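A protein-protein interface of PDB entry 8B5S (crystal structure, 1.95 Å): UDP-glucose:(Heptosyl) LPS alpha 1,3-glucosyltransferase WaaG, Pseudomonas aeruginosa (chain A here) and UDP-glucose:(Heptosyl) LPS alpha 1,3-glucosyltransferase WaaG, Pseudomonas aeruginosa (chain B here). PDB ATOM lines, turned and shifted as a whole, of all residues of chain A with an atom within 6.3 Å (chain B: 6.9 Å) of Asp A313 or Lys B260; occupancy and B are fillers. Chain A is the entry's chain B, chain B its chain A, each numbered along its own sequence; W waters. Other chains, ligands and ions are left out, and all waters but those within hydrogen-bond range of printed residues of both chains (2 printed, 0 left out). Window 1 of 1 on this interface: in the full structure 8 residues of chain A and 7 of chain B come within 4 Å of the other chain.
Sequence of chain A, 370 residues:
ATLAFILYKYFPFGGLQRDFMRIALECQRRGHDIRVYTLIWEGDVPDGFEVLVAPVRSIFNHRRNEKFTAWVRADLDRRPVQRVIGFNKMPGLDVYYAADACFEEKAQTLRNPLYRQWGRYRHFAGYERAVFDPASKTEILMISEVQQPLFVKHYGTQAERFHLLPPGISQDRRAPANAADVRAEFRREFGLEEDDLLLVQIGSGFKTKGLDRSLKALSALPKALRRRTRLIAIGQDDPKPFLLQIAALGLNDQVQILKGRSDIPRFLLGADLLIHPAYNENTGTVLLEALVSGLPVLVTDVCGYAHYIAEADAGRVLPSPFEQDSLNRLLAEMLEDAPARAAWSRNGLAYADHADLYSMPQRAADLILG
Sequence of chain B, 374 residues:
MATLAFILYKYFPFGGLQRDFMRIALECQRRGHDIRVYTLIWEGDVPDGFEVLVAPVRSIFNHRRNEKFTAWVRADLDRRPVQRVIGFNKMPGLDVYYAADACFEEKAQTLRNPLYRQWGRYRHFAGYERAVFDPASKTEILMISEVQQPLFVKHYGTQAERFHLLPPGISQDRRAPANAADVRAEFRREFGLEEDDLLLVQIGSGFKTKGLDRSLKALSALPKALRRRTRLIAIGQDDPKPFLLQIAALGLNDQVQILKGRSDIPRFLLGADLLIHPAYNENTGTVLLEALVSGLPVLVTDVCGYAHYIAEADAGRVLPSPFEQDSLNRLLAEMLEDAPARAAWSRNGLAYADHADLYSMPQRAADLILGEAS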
ATOM      1  N   TYR A 308     -22.134 -23.266  24.043  1.00  0.00           N
ATOM      2  CA  TYR A 308     -22.083 -22.743  22.684  1.00  0.00           C
ATOM      3  C   TYR A 308     -22.795 -21.392  22.583  1.00  0.00           C
ATOM      4  O   TYR A 308     -22.345 -20.506  21.859  1.00  0.00           O
ATOM      5  CB  TYR A 308     -22.702 -23.744  21.706  1.00  0.00           C
ATOM      6  CG  TYR A 308     -21.837 -24.933  21.373  1.00  0.00           C
ATOM      7  CD1 TYR A 308     -20.649 -24.768  20.678  1.00  0.00           C
ATOM      8  CD2 TYR A 308     -22.210 -26.223  21.722  1.00  0.00           C
ATOM      9  CE1 TYR A 308     -19.846 -25.849  20.349  1.00  0.00           C
ATOM     10  CE2 TYR A 308     -21.424 -27.317  21.390  1.00  0.00           C
ATOM     11  CZ  TYR A 308     -20.234 -27.128  20.706  1.00  0.00           C
ATOM     12  OH  TYR A 308     -19.421 -28.185  20.367  1.00  0.00           O
ATOM     13  N   ILE A 309     -23.912 -21.245  23.305  1.00  0.00           N
ATOM     14  CA  ILE A 309     -24.694 -20.017  23.275  1.00  0.00           C
ATOM     15  C   ILE A 309     -23.856 -18.863  23.819  1.00  0.00           C
ATOM     16  O   ILE A 309     -23.842 -17.781  23.233  1.00  0.00           O
ATOM     17  CB  ILE A 309     -26.012 -20.185  24.062  1.00  0.00           C
ATOM     18  CG1 ILE A 309     -26.854 -21.347  23.522  1.00  0.00           C
ATOM     19  CG2 ILE A 309     -26.798 -18.881  24.084  1.00  0.00           C
ATOM     20  CD1 ILE A 309     -27.160 -21.253  22.040  1.00  0.00           C
ATOM     21  N   ALA A 310     -23.180 -19.098  24.951  1.00  0.00           N
ATOM     22  CA  ALA A 310     -22.340 -18.083  25.569  1.00  0.00           C
ATOM     23  C   ALA A 310     -21.149 -17.780  24.663  1.00  0.00           C
ATOM     24  O   ALA A 310     -20.844 -16.618  24.411  1.00  0.00           O
ATOM     25  CB  ALA A 310     -21.898 -18.534  26.939  1.00  0.00           C
ATOM     26  N   GLU A 311     -20.521 -18.837  24.133  1.00  0.00           N
ATOM     27  CA  GLU A 311     -19.316 -18.706  23.329  1.00  0.00           C
ATOM     28  C   GLU A 311     -19.608 -17.951  22.029  1.00  0.00           C
ATOM     29  O   GLU A 311     -18.756 -17.205  21.553  1.00  0.00           O
ATOM     30  CB  GLU A 311     -18.712 -20.091  23.081  1.00  0.00           C
ATOM     31  CG  GLU A 311     -18.071 -20.685  24.332  1.00  0.00           C
ATOM     32  CD  GLU A 311     -17.913 -22.199  24.370  1.00  0.00           C
ATOM     33  OE1 GLU A 311     -18.226 -22.860  23.359  1.00  0.00           O
ATOM     34  OE2 GLU A 311     -17.497 -22.722  25.430  1.00  0.00           O
ATOM     35  N   ALA A 312     -20.816 -18.125  21.475  1.00  0.00           N
ATOM     36  CA  ALA A 312     -21.205 -17.474  20.232  1.00  0.00           C
ATOM     37  C   ALA A 312     -21.810 -16.089  20.479  1.00  0.00           C
ATOM     38  O   ALA A 312     -22.008 -15.337  19.529  1.00  0.00           O
ATOM     39  CB  ALA A 312     -22.179 -18.354  19.487  1.00  0.00           C
ATOM     40  N   ASP A 313     -22.111 -15.762  21.741  1.00  0.00           N
ATOM     41  CA  ASP A 313     -22.835 -14.545  22.098  1.00  0.00           C
ATOM     42  C   ASP A 313     -24.167 -14.527  21.348  1.00  0.00           C
ATOM     43  O   ASP A 313     -24.518 -13.536  20.709  1.00  0.00           O
ATOM     44  CB  ASP A 313     -21.993 -13.289  21.837  1.00  0.00           C
ATOM     45  CG  ASP A 313     -22.566 -12.007  22.427  1.00  0.00           C
ATOM     46  OD1 ASP A 313     -23.479 -12.097  23.268  1.00  0.00           O
ATOM     47  OD2 ASP A 313     -22.106 -10.918  22.028  1.00  0.00           O
ATOM     48  N   ALA A 314     -24.909 -15.635  21.452  1.00  0.00           N
ATOM     49  CA  ALA A 314     -26.116 -15.854  20.665  1.00  0.00           C
ATOM     50  C   ALA A 314     -27.325 -16.024  21.581  1.00  0.00           C
ATOM     51  O   ALA A 314     -28.314 -16.651  21.200  1.00  0.00           O
ATOM     52  CB  ALA A 314     -25.920 -17.067  19.783  1.00  0.00           C
ATOM     53  N   GLY A 315     -27.242 -15.444  22.784  1.00  0.00           N
ATOM     54  CA  GLY A 315     -28.320 -15.509  23.754  1.00  0.00           C
ATOM     55  C   GLY A 315     -27.801 -15.355  25.180  1.00  0.00           C
ATOM     56  O   GLY A 315     -26.762 -14.736  25.400  1.00  0.00           O
ATOM     57  N   ARG A 316     -28.535 -15.927  26.140  1.00  0.00           N
ATOM     58  CA  ARG A 316     -28.171 -15.838  27.545  1.00  0.00           C
ATOM     59  C   ARG A 316     -28.276 -17.213  28.201  1.00  0.00           C
ATOM     60  O   ARG A 316     -29.222 -17.955  27.950  1.00  0.00           O
ATOM     61  CB  ARG A 316     -29.070 -14.825  28.257  1.00  0.00           C
ATOM     62  CG  ARG A 316     -28.722 -13.374  27.957  1.00  0.00           C
ATOM     63  CD  ARG A 316     -27.430 -12.956  28.632  1.00  0.00           C
ATOM     64  NE  ARG A 316     -27.068 -11.593  28.278  1.00  0.00           N
ATOM     65  CZ  ARG A 316     -25.890 -11.214  27.792  1.00  0.00           C
ATOM     66  NH1 ARG A 316     -24.906 -12.084  27.656  1.00  0.00           N
ATOM     67  NH2 ARG A 316     -25.701  -9.956  27.438  1.00  0.00           N
ATOM     68  N   ALA A 343     -28.589  -8.374  17.826  1.00  0.00           N
ATOM     69  CA  ALA A 343     -27.171  -8.703  17.883  1.00  0.00           C
ATOM     70  C   ALA A 343     -26.976 -10.203  18.113  1.00  0.00           C
ATOM     71  O   ALA A 343     -26.119 -10.818  17.483  1.00  0.00           O
ATOM     72  CB  ALA A 343     -26.489  -7.881  18.949  1.00  0.00           C
ATOM     73  N   TRP A 344     -27.775 -10.799  19.008  1.00  0.00           N
ATOM     74  CA  TRP A 344     -27.677 -12.230  19.271  1.00  0.00           C
ATOM     75  C   TRP A 344     -27.942 -13.032  17.995  1.00  0.00           C
ATOM     76  O   TRP A 344     -27.300 -14.054  17.770  1.00  0.00           O
ATOM     77  CB  TRP A 344     -28.599 -12.661  20.423  1.00  0.00           C
ATOM     78  CG  TRP A 344     -28.202 -12.120  21.766  1.00  0.00           C
ATOM     79  CD1 TRP A 344     -26.933 -11.981  22.251  1.00  0.00           C
ATOM     80  CD2 TRP A 344     -29.077 -11.672  22.820  1.00  0.00           C
ATOM     81  NE1 TRP A 344     -26.956 -11.458  23.515  1.00  0.00           N
ATOM     82  CE2 TRP A 344     -28.256 -11.258  23.894  1.00  0.00           C
ATOM     83  CE3 TRP A 344     -30.465 -11.565  22.962  1.00  0.00           C
ATOM     84  CZ2 TRP A 344     -28.778 -10.750  25.082  1.00  0.00           C
ATOM     85  CZ3 TRP A 344     -30.980 -11.059  24.136  1.00  0.00           C
ATOM     86  CH2 TRP A 344     -30.145 -10.653  25.179  1.00  0.00           C
ATOM     87  N   SER A 345     -28.877 -12.543  17.169  1.00  0.00           N
ATOM     88  CA  SER A 345     -29.229 -13.174  15.905  1.00  0.00           C
ATOM     89  C   SER A 345     -28.045 -13.148  14.940  1.00  0.00           C
ATOM     90  O   SER A 345     -27.638 -14.192  14.430  1.00  0.00           O
ATOM     91  CB  SER A 345     -30.442 -12.509  15.304  1.00  0.00           C
ATOM     92  OG  SER A 345     -30.822 -13.141  14.091  1.00  0.00           O
ATOM     93  N   ASN A 347     -24.944 -12.695  15.629  1.00  0.00           N
ATOM     94  CA  ASN A 347     -23.807 -13.398  16.205  1.00  0.00           C
ATOM     95  C   ASN A 347     -23.943 -14.903  15.986  1.00  0.00           C
ATOM     96  O   ASN A 347     -22.952 -15.583  15.723  1.00  0.00           O
ATOM     97  CB  ASN A 347     -23.652 -13.090  17.696  1.00  0.00           C
ATOM     98  CG  ASN A 347     -23.380 -11.628  17.991  1.00  0.00           C
ATOM     99  OD1 ASN A 347     -23.029 -10.857  17.101  1.00  0.00           O
ATOM    100  ND2 ASN A 347     -23.530 -11.240  19.247  1.00  0.00           N
ATOM    101  N   GLY A 348     -25.170 -15.420  16.116  1.00  0.00           N
ATOM    102  CA  GLY A 348     -25.435 -16.831  15.884  1.00  0.00           C
ATOM    103  C   GLY A 348     -25.109 -17.241  14.449  1.00  0.00           C
ATOM    104  O   GLY A 348     -24.404 -18.221  14.227  1.00  0.00           O
ATOM    105  N   TYR A 351     -21.392 -17.195  13.867  1.00  0.00           N
ATOM    106  CA  TYR A 351     -20.801 -18.361  14.504  1.00  0.00           C
ATOM    107  C   TYR A 351     -21.067 -19.619  13.676  1.00  0.00           C
ATOM    108  O   TYR A 351     -20.186 -20.459  13.514  1.00  0.00           O
ATOM    109  CB  TYR A 351     -21.365 -18.531  15.917  1.00  0.00           C
ATOM    110  CG  TYR A 351     -20.670 -19.578  16.748  1.00  0.00           C
ATOM    111  CD1 TYR A 351     -19.433 -19.328  17.321  1.00  0.00           C
ATOM    112  CD2 TYR A 351     -21.240 -20.826  16.954  1.00  0.00           C
ATOM    113  CE1 TYR A 351     -18.785 -20.284  18.087  1.00  0.00           C
ATOM    114  CE2 TYR A 351     -20.605 -21.794  17.717  1.00  0.00           C
ATOM    115  CZ  TYR A 351     -19.371 -21.523  18.282  1.00  0.00           C
ATOM    116  OH  TYR A 351     -18.730 -22.467  19.045  1.00  0.00           O
ATOM    117  N   PHE B  14      -8.686 -12.478  14.528  1.00  0.00           N
ATOM    118  CA  PHE B  14      -8.544 -11.172  15.161  1.00  0.00           C
ATOM    119  C   PHE B  14      -7.889 -11.282  16.539  1.00  0.00           C
ATOM    120  O   PHE B  14      -8.500 -10.963  17.560  1.00  0.00           O
ATOM    121  CB  PHE B  14      -9.901 -10.464  15.230  1.00  0.00           C
ATOM    122  CG  PHE B  14     -10.627 -10.354  13.911  1.00  0.00           C
ATOM    123  CD1 PHE B  14      -9.944 -10.081  12.733  1.00  0.00           C
ATOM    124  CD2 PHE B  14     -12.005 -10.502  13.851  1.00  0.00           C
ATOM    125  CE1 PHE B  14     -10.621  -9.976  11.527  1.00  0.00           C
ATOM    126  CE2 PHE B  14     -12.680 -10.400  12.643  1.00  0.00           C
ATOM    127  CZ  PHE B  14     -11.988 -10.132  11.484  1.00  0.00           C
ATOM    128  N   PHE B 207     -11.989  -6.393  26.351  1.00  0.00           N
ATOM    129  CA  PHE B 207     -12.190  -4.982  26.632  1.00  0.00           C
ATOM    130  C   PHE B 207     -11.895  -4.664  28.097  1.00  0.00           C
ATOM    131  O   PHE B 207     -11.351  -3.603  28.394  1.00  0.00           O
ATOM    132  CB  PHE B 207     -13.615  -4.547  26.277  1.00  0.00           C
ATOM    133  CG  PHE B 207     -13.975  -4.547  24.810  1.00  0.00           C
ATOM    134  CD1 PHE B 207     -13.071  -4.144  23.839  1.00  0.00           C
ATOM    135  CD2 PHE B 207     -15.259  -4.888  24.411  1.00  0.00           C
ATOM    136  CE1 PHE B 207     -13.433  -4.119  22.501  1.00  0.00           C
ATOM    137  CE2 PHE B 207     -15.621  -4.857  23.072  1.00  0.00           C
ATOM    138  CZ  PHE B 207     -14.707  -4.473  22.120  1.00  0.00           C
ATOM    139  N   ALA B 234     -15.345   1.047  19.962  1.00  0.00           N
ATOM    140  CA  ALA B 234     -14.611  -0.119  20.425  1.00  0.00           C
ATOM    141  C   ALA B 234     -14.862  -1.272  19.457  1.00  0.00           C
ATOM    142  O   ALA B 234     -15.974  -1.422  18.951  1.00  0.00           O
ATOM    143  CB  ALA B 234     -15.026  -0.473  21.832  1.00  0.00           C
ATOM    144  N   ILE B 235     -13.817  -2.064  19.191  1.00  0.00           N
ATOM    145  CA  ILE B 235     -13.887  -3.129  18.203  1.00  0.00           C
ATOM    146  C   ILE B 235     -13.304  -4.405  18.803  1.00  0.00           C
ATOM    147  O   ILE B 235     -12.111  -4.477  19.094  1.00  0.00           O
ATOM    148  CB  ILE B 235     -13.170  -2.728  16.898  1.00  0.00           C
ATOM    149  CG1 ILE B 235     -13.729  -1.424  16.315  1.00  0.00           C
ATOM    150  CG2 ILE B 235     -13.223  -3.873  15.897  1.00  0.00           C
ATOM    151  CD1 ILE B 235     -12.979  -0.910  15.098  1.00  0.00           C
ATOM    152  N   GLY B 236     -14.166  -5.413  18.973  1.00  0.00           N
ATOM    153  CA  GLY B 236     -13.763  -6.686  19.548  1.00  0.00           C
ATOM    154  C   GLY B 236     -14.926  -7.670  19.597  1.00  0.00           C
ATOM    155  O   GLY B 236     -16.072  -7.288  19.375  1.00  0.00           O
ATOM    156  N   GLN B 237     -14.612  -8.933  19.907  1.00  0.00           N
ATOM    157  CA  GLN B 237     -15.573 -10.025  19.838  1.00  0.00           C
ATOM    158  C   GLN B 237     -16.373 -10.152  21.133  1.00  0.00           C
ATOM    159  O   GLN B 237     -17.326 -10.930  21.186  1.00  0.00           O
ATOM    160  CB  GLN B 237     -14.854 -11.342  19.535  1.00  0.00           C
ATOM    161  CG  GLN B 237     -14.428 -11.477  18.082  1.00  0.00           C
ATOM    162  CD  GLN B 237     -15.620 -11.412  17.158  1.00  0.00           C
ATOM    163  OE1 GLN B 237     -15.849 -10.413  16.488  1.00  0.00           O
ATOM    164  NE2 GLN B 237     -16.421 -12.464  17.149  1.00  0.00           N
ATOM    165  N   ASP B 238     -15.986  -9.380  22.160  1.00  0.00           N
ATOM    166  CA  ASP B 238     -16.581  -9.449  23.486  1.00  0.00           C
ATOM    167  C   ASP B 238     -18.094  -9.280  23.430  1.00  0.00           C
ATOM    168  O   ASP B 238     -18.619  -8.614  22.539  1.00  0.00           O
ATOM    169  CB  ASP B 238     -16.073  -8.327  24.393  1.00  0.00           C
ATOM    170  CG  ASP B 238     -14.573  -8.322  24.612  1.00  0.00           C
ATOM    171  OD1 ASP B 238     -13.830  -8.428  23.609  1.00  0.00           O
ATOM    172  OD2 ASP B 238     -14.163  -8.183  25.777  1.00  0.00           O
ATOM    173  N   ASP B 239     -18.772  -9.860  24.427  1.00  0.00           N
ATOM    174  CA  ASP B 239     -20.143  -9.506  24.749  1.00  0.00           C
ATOM    175  C   ASP B 239     -20.155  -8.034  25.159  1.00  0.00           C
ATOM    176  O   ASP B 239     -19.473  -7.653  26.108  1.00  0.00           O
ATOM    177  CB  ASP B 239     -20.694 -10.430  25.842  1.00  0.00           C
ATOM    178  CG  ASP B 239     -22.046 -10.031  26.412  1.00  0.00           C
ATOM    179  OD1 ASP B 239     -22.641  -9.057  25.908  1.00  0.00           O
ATOM    180  OD2 ASP B 239     -22.488 -10.693  27.376  1.00  0.00           O
ATOM    181  N   PRO B 240     -20.892  -7.151  24.446  1.00  0.00           N
ATOM    182  CA  PRO B 240     -20.890  -5.722  24.767  1.00  0.00           C
ATOM    183  C   PRO B 240     -21.734  -5.285  25.965  1.00  0.00           C
ATOM    184  O   PRO B 240     -21.557  -4.167  26.443  1.00  0.00           O
ATOM    185  CB  PRO B 240     -21.440  -5.088  23.480  1.00  0.00           C
ATOM    186  CG  PRO B 240     -22.362  -6.142  22.907  1.00  0.00           C
ATOM    187  CD  PRO B 240     -21.708  -7.463  23.261  1.00  0.00           C
ATOM    188  N   LYS B 241     -22.616  -6.164  26.468  1.00  0.00           N
ATOM    189  CA  LYS B 241     -23.670  -5.753  27.389  1.00  0.00           C
ATOM    190  C   LYS B 241     -23.102  -5.052  28.625  1.00  0.00           C
ATOM    191  O   LYS B 241     -23.639  -4.024  29.031  1.00  0.00           O
ATOM    192  CB  LYS B 241     -24.554  -6.925  27.829  1.00  0.00           C
ATOM    193  CG  LYS B 241     -25.782  -6.521  28.645  1.00  0.00           C
ATOM    194  CD  LYS B 241     -26.352  -7.606  29.549  1.00  0.00           C
ATOM    195  CE  LYS B 241     -25.783  -7.613  30.955  1.00  0.00           C
ATOM    196  NZ  LYS B 241     -24.308  -7.769  30.979  1.00  0.00           N
ATOM    197  N   ILE B 258     -20.001  -0.050  20.117  1.00  0.00           N
ATOM    198  CA  ILE B 258     -19.166  -1.218  20.348  1.00  0.00           C
ATOM    199  C   ILE B 258     -19.431  -2.211  19.219  1.00  0.00           C
ATOM    200  O   ILE B 258     -20.521  -2.771  19.122  1.00  0.00           O
ATOM    201  CB  ILE B 258     -19.419  -1.815  21.747  1.00  0.00           C
ATOM    202  CG1 ILE B 258     -19.280  -0.746  22.836  1.00  0.00           C
ATOM    203  CG2 ILE B 258     -18.499  -3.003  22.005  1.00  0.00           C
ATOM    204  CD1 ILE B 258     -19.576  -1.241  24.226  1.00  0.00           C
ATOM    205  N   LEU B 259     -18.416  -2.402  18.369  1.00  0.00           N
ATOM    206  CA  LEU B 259     -18.547  -3.198  17.161  1.00  0.00           C
ATOM    207  C   LEU B 259     -17.872  -4.552  17.369  1.00  0.00           C
ATOM    208  O   LEU B 259     -16.910  -4.664  18.129  1.00  0.00           O
ATOM    209  CB  LEU B 259     -17.896  -2.443  15.998  1.00  0.00           C
ATOM    210  CG  LEU B 259     -18.347  -0.996  15.799  1.00  0.00           C
ATOM    211  CD1 LEU B 259     -17.704  -0.405  14.554  1.00  0.00           C
ATOM    212  CD2 LEU B 259     -19.859  -0.896  15.716  1.00  0.00           C
ATOM    213  N   LYS B 260     -18.390  -5.571  16.672  1.00  0.00           N
ATOM    214  CA  LYS B 260     -17.762  -6.881  16.639  1.00  0.00           C
ATOM    215  C   LYS B 260     -16.478  -6.804  15.815  1.00  0.00           C
ATOM    216  O   LYS B 260     -16.241  -5.821  15.115  1.00  0.00           O
ATOM    217  CB  LYS B 260     -18.740  -7.923  16.086  1.00  0.00           C
ATOM    218  CG  LYS B 260     -19.842  -8.332  17.054  1.00  0.00           C
ATOM    219  CD  LYS B 260     -19.362  -9.221  18.185  1.00  0.00           C
ATOM    220  CE  LYS B 260     -20.440  -9.481  19.213  1.00  0.00           C
ATOM    221  NZ  LYS B 260     -20.046 -10.530  20.181  1.00  0.00           N
ATOM    222  N   GLY B 261     -15.649  -7.847  15.932  1.00  0.00           N
ATOM    223  CA  GLY B 261     -14.371  -7.912  15.242  1.00  0.00           C
ATOM    224  C   GLY B 261     -14.537  -7.757  13.732  1.00  0.00           C
ATOM    225  O   GLY B 261     -15.547  -8.172  13.167  1.00  0.00           O
ATOM    226  N   ARG B 262     -13.543  -7.139  13.086  1.00  0.00           N
ATOM    227  CA  ARG B 262     -13.614  -6.893  11.655  1.00  0.00           C
ATOM    228  C   ARG B 262     -12.207  -6.708  11.099  1.00  0.00           C
ATOM    229  O   ARG B 262     -11.271  -6.409  11.838  1.00  0.00           O
ATOM    230  CB  ARG B 262     -14.518  -5.690  11.368  1.00  0.00           C
ATOM    231  CG  ARG B 262     -14.262  -4.476  12.251  1.00  0.00           C
ATOM    232  CD  ARG B 262     -15.439  -3.521  12.196  1.00  0.00           C
ATOM    233  NE  ARG B 262     -15.605  -2.971  10.858  1.00  0.00           N
ATOM    234  CZ  ARG B 262     -16.741  -2.500  10.361  1.00  0.00           C
ATOM    235  NH1 ARG B 262     -17.863  -2.587  11.055  1.00  0.00           N
ATOM    236  NH2 ARG B 262     -16.758  -1.974   9.149  1.00  0.00           N
ATOM    237  N   SER B 263     -12.083  -6.880   9.780  1.00  0.00           N
ATOM    238  CA  SER B 263     -10.782  -6.954   9.137  1.00  0.00           C
ATOM    239  C   SER B 263     -10.302  -5.582   8.654  1.00  0.00           C
ATOM    240  O   SER B 263      -9.114  -5.426   8.373  1.00  0.00           O
ATOM    241  CB  SER B 263     -10.804  -7.974   8.023  1.00  0.00           C
ATOM    242  OG  SER B 263     -11.856  -7.712   7.107  1.00  0.00           O
HETATM  243  O   HOH W   1     -19.844 -12.905  18.740  1.00  0.00           O
HETATM  244  O   HOH W   2     -24.553  -9.784  24.167  1.00  0.00           O
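The guanidinium group (NH1) of Arg A316 lies within salt-bridge range of the side-chain carboxylate (OD2) of Asp B239 (2.8 Å).
The side-chain amino group of Lys B260 is in salt-bridge range of the side-chain carboxylate of Asp A313, 2.8 Å away.
Among the printed residues, merely in contact across the chains: Arg A316 with Lys B241 (3.2 Å), Asn A347 with Lys B260 (3.6 Å), Asp A313 with Asp B239 (3.6 Å) and Asp A313 with Pro B240 (3.7 Å).
Water W2 lies within hydrogen-bond range of OD1 of Asp B239, OD1 of Asp A313, NE1 of Trp A344 and NH2 of Arg A316.
Water W1 bridges NZ of Lys B260 and O of Ala A312.
O of Gln B237 sits at hydrogen-bond distance from NZ of Lys B260.
The side-chain amino group of Lys B260 lies within hydrogen-bond range of the backbone carbonyl oxygen of Asp B238 (3.4 Å).
The backbone NH of Lys B241 sits at hydrogen-bond distance from the side-chain carboxylate of Asp B239 (2.9 Å).
The side-chain amide nitrogen of Asn A347 sits at hydrogen-bond distance from the backbone carbonyl oxygen of Asp A313, 2.9 Å away.
O of Ala A343 lies close to OD1 of Asn A347 (3.1 Å).
Of chain B, only Asp B239, Pro B240 and Lys B260 come within 4 Å of Asp A313.
Of the printed residues of chain B, Arg A316 touches Asp B239 and Lys B241.
Printed residues of chain A within 4 Å of Asp B239: Asp A313 (3.6 Å) and Arg A316 (2.8 Å).
Of the printed residues of chain A, Lys B241 touches Arg A316 (3.2 Å).
Ile B258 touches none of the printed residues of chain A.
Lys B260 touches just these residues of chain A: Asp A313 and Asn A347.
Along chain A the printed residues that touch a printed residue of chain B span positions 313 to 347.
Printed residues of chain B that touch a printed residue of chain A: Asp B239, Pro B240, Lys B241 and Lys B260.
Hydrophobic or aromatic side chains of chain B that line the printed part of chain A: Pro B240.
Among the printed residues, 6 pairs touch across the chains.
Among the printed residues, Asp or Glu carboxylates within 4 Å of a Lys or Arg side-chain nitrogen of the other chain: Asp A313 with Lys B260 (2.8 Å) and Arg A316 with Asp B239 (2.8 Å).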
